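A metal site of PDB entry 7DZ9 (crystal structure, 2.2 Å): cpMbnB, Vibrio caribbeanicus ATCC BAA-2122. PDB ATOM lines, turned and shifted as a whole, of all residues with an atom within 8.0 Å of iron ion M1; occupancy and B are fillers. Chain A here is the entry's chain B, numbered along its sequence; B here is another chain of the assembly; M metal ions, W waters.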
ATOM      1  N   HIS A  55      -1.961  -4.628   7.414  1.00  0.00           N
ATOM      2  CA  HIS A  55      -1.275  -4.793   6.142  1.00  0.00           C
ATOM      3  C   HIS A  55      -2.334  -4.735   5.058  1.00  0.00           C
ATOM      4  O   HIS A  55      -3.339  -5.443   5.146  1.00  0.00           O
ATOM      5  CB  HIS A  55      -0.522  -6.127   6.144  1.00  0.00           C
ATOM      6  CG  HIS A  55       0.517  -6.275   5.075  1.00  0.00           C
ATOM      7  ND1 HIS A  55       1.422  -5.287   4.759  1.00  0.00           N
ATOM      8  CD2 HIS A  55       0.807  -7.326   4.267  1.00  0.00           C
ATOM      9  CE1 HIS A  55       2.214  -5.700   3.790  1.00  0.00           C
ATOM     10  NE2 HIS A  55       1.867  -6.941   3.477  1.00  0.00           N
ATOM     11  N   HIS A  91       1.548  -2.062  -0.159  1.00  0.00           N
ATOM     12  CA  HIS A  91       2.533  -2.570  -1.105  1.00  0.00           C
ATOM     13  C   HIS A  91       2.722  -1.575  -2.227  1.00  0.00           C
ATOM     14  O   HIS A  91       1.851  -0.744  -2.505  1.00  0.00           O
ATOM     15  CB  HIS A  91       2.129  -3.901  -1.730  1.00  0.00           C
ATOM     16  CG  HIS A  91       1.919  -5.021  -0.763  1.00  0.00           C
ATOM     17  ND1 HIS A  91       0.779  -5.158  -0.016  1.00  0.00           N
ATOM     18  CD2 HIS A  91       2.711  -6.075  -0.452  1.00  0.00           C
ATOM     19  CE1 HIS A  91       0.868  -6.238   0.736  1.00  0.00           C
ATOM     20  NE2 HIS A  91       2.030  -6.814   0.495  1.00  0.00           N
ATOM     21  N   GLU A 135       5.993  -1.965   1.768  1.00  0.00           N
ATOM     22  CA  GLU A 135       6.789  -3.187   1.795  1.00  0.00           C
ATOM     23  C   GLU A 135       7.616  -3.331   0.521  1.00  0.00           C
ATOM     24  O   GLU A 135       7.130  -3.057  -0.570  1.00  0.00           O
ATOM     25  CB  GLU A 135       5.871  -4.394   1.963  1.00  0.00           C
ATOM     26  CG  GLU A 135       6.622  -5.710   2.109  1.00  0.00           C
ATOM     27  CD  GLU A 135       5.697  -6.905   2.277  1.00  0.00           C
ATOM     28  OE1 GLU A 135       4.482  -6.790   1.992  1.00  0.00           O
ATOM     29  OE2 GLU A 135       6.182  -7.976   2.700  1.00  0.00           O
ATOM     30  N   ASN A 136       8.865  -3.768   0.662  1.00  0.00           N
ATOM     31  CA  ASN A 136       9.694  -4.087  -0.499  1.00  0.00           C
ATOM     32  C   ASN A 136       9.174  -5.322  -1.223  1.00  0.00           C
ATOM     33  O   ASN A 136       8.709  -6.281  -0.594  1.00  0.00           O
ATOM     34  CB  ASN A 136      11.170  -4.290  -0.106  1.00  0.00           C
ATOM     35  CG  ASN A 136      11.357  -5.275   1.029  1.00  0.00           C
ATOM     36  OD1 ASN A 136      10.832  -5.086   2.130  1.00  0.00           O
ATOM     37  ND2 ASN A 136      12.128  -6.330   0.774  1.00  0.00           N
ATOM     38  N   TYR A 137       9.246  -5.308  -2.556  1.00  0.00           N
ATOM     39  CA  TYR A 137       8.740  -6.354  -3.450  1.00  0.00           C
ATOM     40  C   TYR A 137       9.785  -7.452  -3.663  1.00  0.00           C
ATOM     41  O   TYR A 137      10.989  -7.170  -3.725  1.00  0.00           O
ATOM     42  CB  TYR A 137       8.360  -5.747  -4.808  1.00  0.00           C
ATOM     43  CG  TYR A 137       7.564  -6.699  -5.714  1.00  0.00           C
ATOM     44  CD1 TYR A 137       8.205  -7.631  -6.518  1.00  0.00           C
ATOM     45  CD2 TYR A 137       6.179  -6.657  -5.730  1.00  0.00           C
ATOM     46  CE1 TYR A 137       7.488  -8.485  -7.331  1.00  0.00           C
ATOM     47  CE2 TYR A 137       5.453  -7.509  -6.545  1.00  0.00           C
ATOM     48  CZ  TYR A 137       6.117  -8.416  -7.333  1.00  0.00           C
ATOM     49  OH  TYR A 137       5.390  -9.269  -8.148  1.00  0.00           O
ATOM     50  N   PRO A 138       9.384  -8.754  -3.755  1.00  0.00           N
ATOM     51  CA  PRO A 138      10.353  -9.847  -4.054  1.00  0.00           C
ATOM     52  C   PRO A 138      10.664  -9.929  -5.559  1.00  0.00           C
ATOM     53  O   PRO A 138      10.204 -10.817  -6.282  1.00  0.00           O
ATOM     54  CB  PRO A 138       9.625 -11.087  -3.543  1.00  0.00           C
ATOM     55  CG  PRO A 138       8.118 -10.760  -3.782  1.00  0.00           C
ATOM     56  CD  PRO A 138       8.009  -9.259  -3.555  1.00  0.00           C
ATOM     57  N   ASP A 165      10.722  -6.554   4.322  1.00  0.00           N
ATOM     58  CA  ASP A 165      10.508  -7.989   4.229  1.00  0.00           C
ATOM     59  C   ASP A 165      11.854  -8.661   3.947  1.00  0.00           C
ATOM     60  O   ASP A 165      12.397  -8.555   2.835  1.00  0.00           O
ATOM     61  CB  ASP A 165       9.465  -8.338   3.166  1.00  0.00           C
ATOM     62  CG  ASP A 165       9.006  -9.771   3.280  1.00  0.00           C
ATOM     63  OD1 ASP A 165       9.874 -10.670   3.207  1.00  0.00           O
ATOM     64  OD2 ASP A 165       7.793 -10.028   3.423  1.00  0.00           O
ATOM     65  N   ILE A 166      12.355  -9.392   4.944  1.00  0.00           N
ATOM     66  CA  ILE A 166      13.706  -9.963   4.873  1.00  0.00           C
ATOM     67  C   ILE A 166      13.780 -11.033   3.796  1.00  0.00           C
ATOM     68  O   ILE A 166      14.755 -11.117   3.044  1.00  0.00           O
ATOM     69  CB  ILE A 166      14.118 -10.507   6.251  1.00  0.00           C
ATOM     70  CG1 ILE A 166      14.131  -9.368   7.277  1.00  0.00           C
ATOM     71  CG2 ILE A 166      15.482 -11.203   6.175  1.00  0.00           C
ATOM     72  CD1 ILE A 166      14.174  -9.889   8.706  1.00  0.00           C
ATOM     73  N   SER A 167      12.755 -11.882   3.698  1.00  0.00           N
ATOM     74  CA  SER A 167      12.842 -12.932   2.696  1.00  0.00           C
ATOM     75  C   SER A 167      12.522 -12.416   1.294  1.00  0.00           C
ATOM     76  O   SER A 167      13.062 -12.938   0.309  1.00  0.00           O
ATOM     77  CB  SER A 167      11.934 -14.110   3.072  1.00  0.00           C
ATOM     78  OG  SER A 167      10.601 -13.706   3.230  1.00  0.00           O
ATOM     79  N   ASN A 168      11.654 -11.396   1.180  1.00  0.00           N
ATOM     80  CA  ASN A 168      11.485 -10.737  -0.123  1.00  0.00           C
ATOM     81  C   ASN A 168      12.813 -10.200  -0.647  1.00  0.00           C
ATOM     82  O   ASN A 168      13.119 -10.322  -1.839  1.00  0.00           O
ATOM     83  CB  ASN A 168      10.459  -9.611  -0.038  1.00  0.00           C
ATOM     84  CG  ASN A 168       9.036 -10.110   0.204  1.00  0.00           C
ATOM     85  OD1 ASN A 168       8.819 -11.281   0.462  1.00  0.00           O
ATOM     86  ND2 ASN A 168       8.079  -9.200   0.148  1.00  0.00           N
ATOM     87  N   ALA A 169      13.599  -9.582   0.228  1.00  0.00           N
ATOM     88  CA  ALA A 169      14.896  -9.049  -0.190  1.00  0.00           C
ATOM     89  C   ALA A 169      15.883 -10.165  -0.507  1.00  0.00           C
ATOM     90  O   ALA A 169      16.686 -10.050  -1.434  1.00  0.00           O
ATOM     91  CB  ALA A 169      15.458  -8.115   0.883  1.00  0.00           C
ATOM     92  N   ILE A 171      14.957 -13.050  -1.732  1.00  0.00           N
ATOM     93  CA  ILE A 171      14.441 -13.510  -3.024  1.00  0.00           C
ATOM     94  C   ILE A 171      14.959 -12.626  -4.147  1.00  0.00           C
ATOM     95  O   ILE A 171      15.384 -13.116  -5.204  1.00  0.00           O
ATOM     96  CB  ILE A 171      12.905 -13.543  -2.993  1.00  0.00           C
ATOM     97  CG1 ILE A 171      12.396 -14.762  -2.233  1.00  0.00           C
ATOM     98  CG2 ILE A 171      12.312 -13.431  -4.390  1.00  0.00           C
ATOM     99  CD1 ILE A 171      10.864 -14.754  -2.005  1.00  0.00           C
ATOM    100  N   HIS A 194       9.068  -8.367   8.160  1.00  0.00           N
ATOM    101  CA  HIS A 194       8.477  -9.627   7.737  1.00  0.00           C
ATOM    102  C   HIS A 194       9.594 -10.633   7.482  1.00  0.00           C
ATOM    103  O   HIS A 194      10.701 -10.267   7.089  1.00  0.00           O
ATOM    104  CB  HIS A 194       7.697  -9.493   6.426  1.00  0.00           C
ATOM    105  CG  HIS A 194       6.364  -8.840   6.557  1.00  0.00           C
ATOM    106  ND1 HIS A 194       5.461  -8.799   5.512  1.00  0.00           N
ATOM    107  CD2 HIS A 194       5.771  -8.198   7.588  1.00  0.00           C
ATOM    108  CE1 HIS A 194       4.367  -8.171   5.903  1.00  0.00           C
ATOM    109  NE2 HIS A 194       4.540  -7.777   7.154  1.00  0.00           N
ATOM    110  N   ILE A 195       9.254 -11.921   7.638  1.00  0.00           N
ATOM    111  CA  ILE A 195      10.121 -13.025   7.257  1.00  0.00           C
ATOM    112  C   ILE A 195       9.238 -14.234   6.952  1.00  0.00           C
ATOM    113  O   ILE A 195       8.212 -14.439   7.616  1.00  0.00           O
ATOM    114  CB  ILE A 195      11.158 -13.328   8.374  1.00  0.00           C
ATOM    115  CG1 ILE A 195      12.310 -14.172   7.850  1.00  0.00           C
ATOM    116  CG2 ILE A 195      10.494 -13.954   9.596  1.00  0.00           C
ATOM    117  CD1 ILE A 195      13.422 -14.317   8.878  1.00  0.00           C
ATOM    118  N   ALA A 196       9.602 -15.002   5.930  1.00  0.00           N
ATOM    119  CA  ALA A 196       8.737 -16.085   5.462  1.00  0.00           C
ATOM    120  C   ALA A 196       9.538 -17.078   4.615  1.00  0.00           C
ATOM    121  O   ALA A 196      10.703 -16.855   4.297  1.00  0.00           O
ATOM    122  CB  ALA A 196       7.563 -15.537   4.658  1.00  0.00           C
ATOM    123  N   GLY A 197       8.875 -18.157   4.188  1.00  0.00           N
ATOM    124  CA  GLY A 197       9.455 -19.116   3.278  1.00  0.00           C
ATOM    125  C   GLY A 197       9.031 -18.861   1.831  1.00  0.00           C
ATOM    126  O   GLY A 197       8.224 -17.990   1.537  1.00  0.00           O
ATOM    127  N   PHE A 198       9.609 -19.646   0.931  1.00  0.00           N
ATOM    128  CA  PHE A 198       9.379 -19.476  -0.494  1.00  0.00           C
ATOM    129  C   PHE A 198       9.591 -20.819  -1.191  1.00  0.00           C
ATOM    130  O   PHE A 198       9.897 -21.822  -0.555  1.00  0.00           O
ATOM    131  CB  PHE A 198      10.276 -18.368  -1.070  1.00  0.00           C
ATOM    132  CG  PHE A 198      11.721 -18.427  -0.604  1.00  0.00           C
ATOM    133  CD1 PHE A 198      12.573 -19.442  -1.024  1.00  0.00           C
ATOM    134  CD2 PHE A 198      12.222 -17.437   0.246  1.00  0.00           C
ATOM    135  CE1 PHE A 198      13.907 -19.473  -0.598  1.00  0.00           C
ATOM    136  CE2 PHE A 198      13.554 -17.468   0.681  1.00  0.00           C
ATOM    137  CZ  PHE A 198      14.401 -18.471   0.251  1.00  0.00           C
ATOM    138  N   VAL A 208       9.898 -17.952  -5.900  1.00  0.00           N
ATOM    139  CA  VAL A 208       8.543 -17.442  -5.822  1.00  0.00           C
ATOM    140  C   VAL A 208       8.219 -17.220  -4.353  1.00  0.00           C
ATOM    141  O   VAL A 208       8.463 -18.106  -3.517  1.00  0.00           O
ATOM    142  CB  VAL A 208       7.516 -18.403  -6.448  1.00  0.00           C
ATOM    143  CG1 VAL A 208       6.137 -17.773  -6.491  1.00  0.00           C
ATOM    144  CG2 VAL A 208       7.978 -18.886  -7.864  1.00  0.00           C
ATOM    145  N   ASP A 209       7.647 -16.070  -4.043  1.00  0.00           N
ATOM    146  CA  ASP A 209       7.404 -15.619  -2.667  1.00  0.00           C
ATOM    147  C   ASP A 209       6.064 -16.201  -2.189  1.00  0.00           C
ATOM    148  O   ASP A 209       5.065 -15.506  -2.062  1.00  0.00           O
ATOM    149  CB  ASP A 209       7.419 -14.086  -2.618  1.00  0.00           C
ATOM    150  CG  ASP A 209       7.184 -13.537  -1.215  1.00  0.00           C
ATOM    151  OD1 ASP A 209       7.730 -14.100  -0.250  1.00  0.00           O
ATOM    152  OD2 ASP A 209       6.462 -12.510  -1.095  1.00  0.00           O
ATOM    153  N   THR A 210       6.067 -17.511  -1.936  1.00  0.00           N
ATOM    154  CA  THR A 210       4.807 -18.223  -1.664  1.00  0.00           C
ATOM    155  C   THR A 210       4.350 -18.136  -0.208  1.00  0.00           C
ATOM    156  O   THR A 210       3.175 -18.402   0.055  1.00  0.00           O
ATOM    157  CB  THR A 210       4.913 -19.701  -2.013  1.00  0.00           C
ATOM    158  OG1 THR A 210       6.009 -20.295  -1.299  1.00  0.00           O
ATOM    159  CG2 THR A 210       5.095 -19.880  -3.508  1.00  0.00           C
ATOM    160  N   HIS A 211       5.234 -17.835   0.750  1.00  0.00           N
ATOM    161  CA  HIS A 211       4.899 -17.915   2.180  1.00  0.00           C
ATOM    162  C   HIS A 211       4.327 -19.295   2.519  1.00  0.00           C
ATOM    163  O   HIS A 211       3.352 -19.428   3.278  1.00  0.00           O
ATOM    164  CB  HIS A 211       3.898 -16.826   2.594  1.00  0.00           C
ATOM    165  CG  HIS A 211       4.328 -15.426   2.259  1.00  0.00           C
ATOM    166  ND1 HIS A 211       3.451 -14.363   2.247  1.00  0.00           N
ATOM    167  CD2 HIS A 211       5.550 -14.908   1.948  1.00  0.00           C
ATOM    168  CE1 HIS A 211       4.104 -13.258   1.918  1.00  0.00           C
ATOM    169  NE2 HIS A 211       5.371 -13.563   1.733  1.00  0.00           N
ATOM    170  N   GLU A 238       5.308 -14.918   8.270  1.00  0.00           N
ATOM    171  CA  GLU A 238       4.155 -15.055   7.391  1.00  0.00           C
ATOM    172  C   GLU A 238       3.946 -16.496   6.931  1.00  0.00           C
ATOM    173  O   GLU A 238       4.907 -17.232   6.671  1.00  0.00           O
ATOM    174  CB  GLU A 238       4.289 -14.160   6.161  1.00  0.00           C
ATOM    175  CG  GLU A 238       4.968 -12.818   6.382  1.00  0.00           C
ATOM    176  CD  GLU A 238       4.767 -11.905   5.179  1.00  0.00           C
ATOM    177  OE1 GLU A 238       5.684 -11.744   4.369  1.00  0.00           O
ATOM    178  OE2 GLU A 238       3.653 -11.393   5.018  1.00  0.00           O
ATOM    179  N   ASP A 240       0.864 -18.488   4.269  1.00  0.00           N
ATOM    180  CA  ASP A 240      -0.370 -18.375   3.520  1.00  0.00           C
ATOM    181  C   ASP A 240      -0.858 -19.681   2.931  1.00  0.00           C
ATOM    182  O   ASP A 240      -1.998 -19.726   2.438  1.00  0.00           O
ATOM    183  CB  ASP A 240      -0.213 -17.341   2.395  1.00  0.00           C
ATOM    184  CG  ASP A 240       0.015 -15.933   2.939  1.00  0.00           C
ATOM    185  OD1 ASP A 240      -0.717 -15.519   3.869  1.00  0.00           O
ATOM    186  OD2 ASP A 240       0.947 -15.274   2.456  1.00  0.00           O
ATOM    187  N   CYS B  18      -0.790 -12.428   0.425  1.00  0.00           N
ATOM    188  CA  CYS B  18       0.448 -11.872  -0.095  1.00  0.00           C
ATOM    189  C   CYS B  18       1.255 -12.952  -0.803  1.00  0.00           C
ATOM    190  O   CYS B  18       2.035 -12.650  -1.703  1.00  0.00           O
ATOM    191  CB  CYS B  18       1.312 -11.306   1.027  1.00  0.00           C
ATOM    192  SG  CYS B  18       0.831  -9.720   1.624  1.00  0.00           S
ATOM    193  N   GLY B  19       1.049 -14.199  -0.414  1.00  0.00           N
ATOM    194  CA  GLY B  19       1.704 -15.327  -1.032  1.00  0.00           C
ATOM    195  C   GLY B  19       1.440 -15.441  -2.520  1.00  0.00           C
ATOM    196  O   GLY B  19       0.282 -15.519  -2.958  1.00  0.00           O
ATOM    197  N   ALA B  20       2.509 -15.418  -3.308  1.00  0.00           N
ATOM    198  CA  ALA B  20       2.381 -15.629  -4.744  1.00  0.00           C
ATOM    199  C   ALA B  20       1.987 -17.075  -5.057  1.00  0.00           C
ATOM    200  O   ALA B  20       2.209 -18.002  -4.269  1.00  0.00           O
ATOM    201  CB  ALA B  20       3.683 -15.253  -5.445  1.00  0.00           C
HETATM  202 FE    FE M   1       6.943 -12.250   1.036  1.00  0.00          FE
HETATM  203 FE    FE M   2       5.736  -9.770   3.419  1.00  0.00          FE
HETATM  204 FE    FE M   3       2.856  -8.223   1.926  1.00  0.00          FE
HETATM  205  O   HOH W   1       7.749 -12.675   2.856  1.00  0.00           O
HETATM  206  O   HOH W   2       5.890 -10.354   1.507  1.00  0.00           O
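N of His 211 is in hydrogen-bond range of O of Gly 197, at 3.1 Å. A ring nitrogen (ND1) of His 211 lies within hydrogen-bond range of the side-chain carboxylate of Asp 240, 2.7 Å away. N of Asn 168 sits at hydrogen-bond distance from OD1 of Asp 165, 2.8 Å away. The side-chain carboxylate of Glu 135 lies close to the side-chain amide nitrogen of Asn 168. The side-chain amide nitrogen of Asn 168 lies within hydrogen-bond range of the backbone carbonyl oxygen of Asn 136. The backbone carbonyl oxygen (O) of Asp 209 is in hydrogen-bond range of the backbone NH (N) of Ala 20 of chain B (2.8 Å). The side-chain carboxylate (OD1) of Asp 165 lies within hydrogen-bond range of the side-chain hydroxyl (OG) of Ser 167. The backbone carbonyl oxygen of Ile 195 sits at hydrogen-bond distance from the backbone NH of Glu 238, 3.0 Å away.
Asp 165 touches iron ion M1. Glu 238 touches iron ion M1 (OE1 to FE, 3.6 Å). Of the 26 residues printed, 5 come within 4 Å of iron ion M1. The nearest printed residue that does not touch iron ion M1 is Ser 167 (4.5 Å).
Iron ion M1 is bound by water W1 (2.0 Å), NE2 of His 211 (2.2 Å), OD1 of Asn 168 (2.2 Å), OD2 of Asp 209 (2.2 Å), water W2 (2.2 Å) and OD1 of Asp 209 (2.4 Å). Iron ion M1 has six donor atoms within binding distance.
Water W1 bridges the side-chain carboxylate (OD1) of Asp 165 (2.9 Å) and the side-chain hydroxyl (OG) of Ser 167 (3.1 Å).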
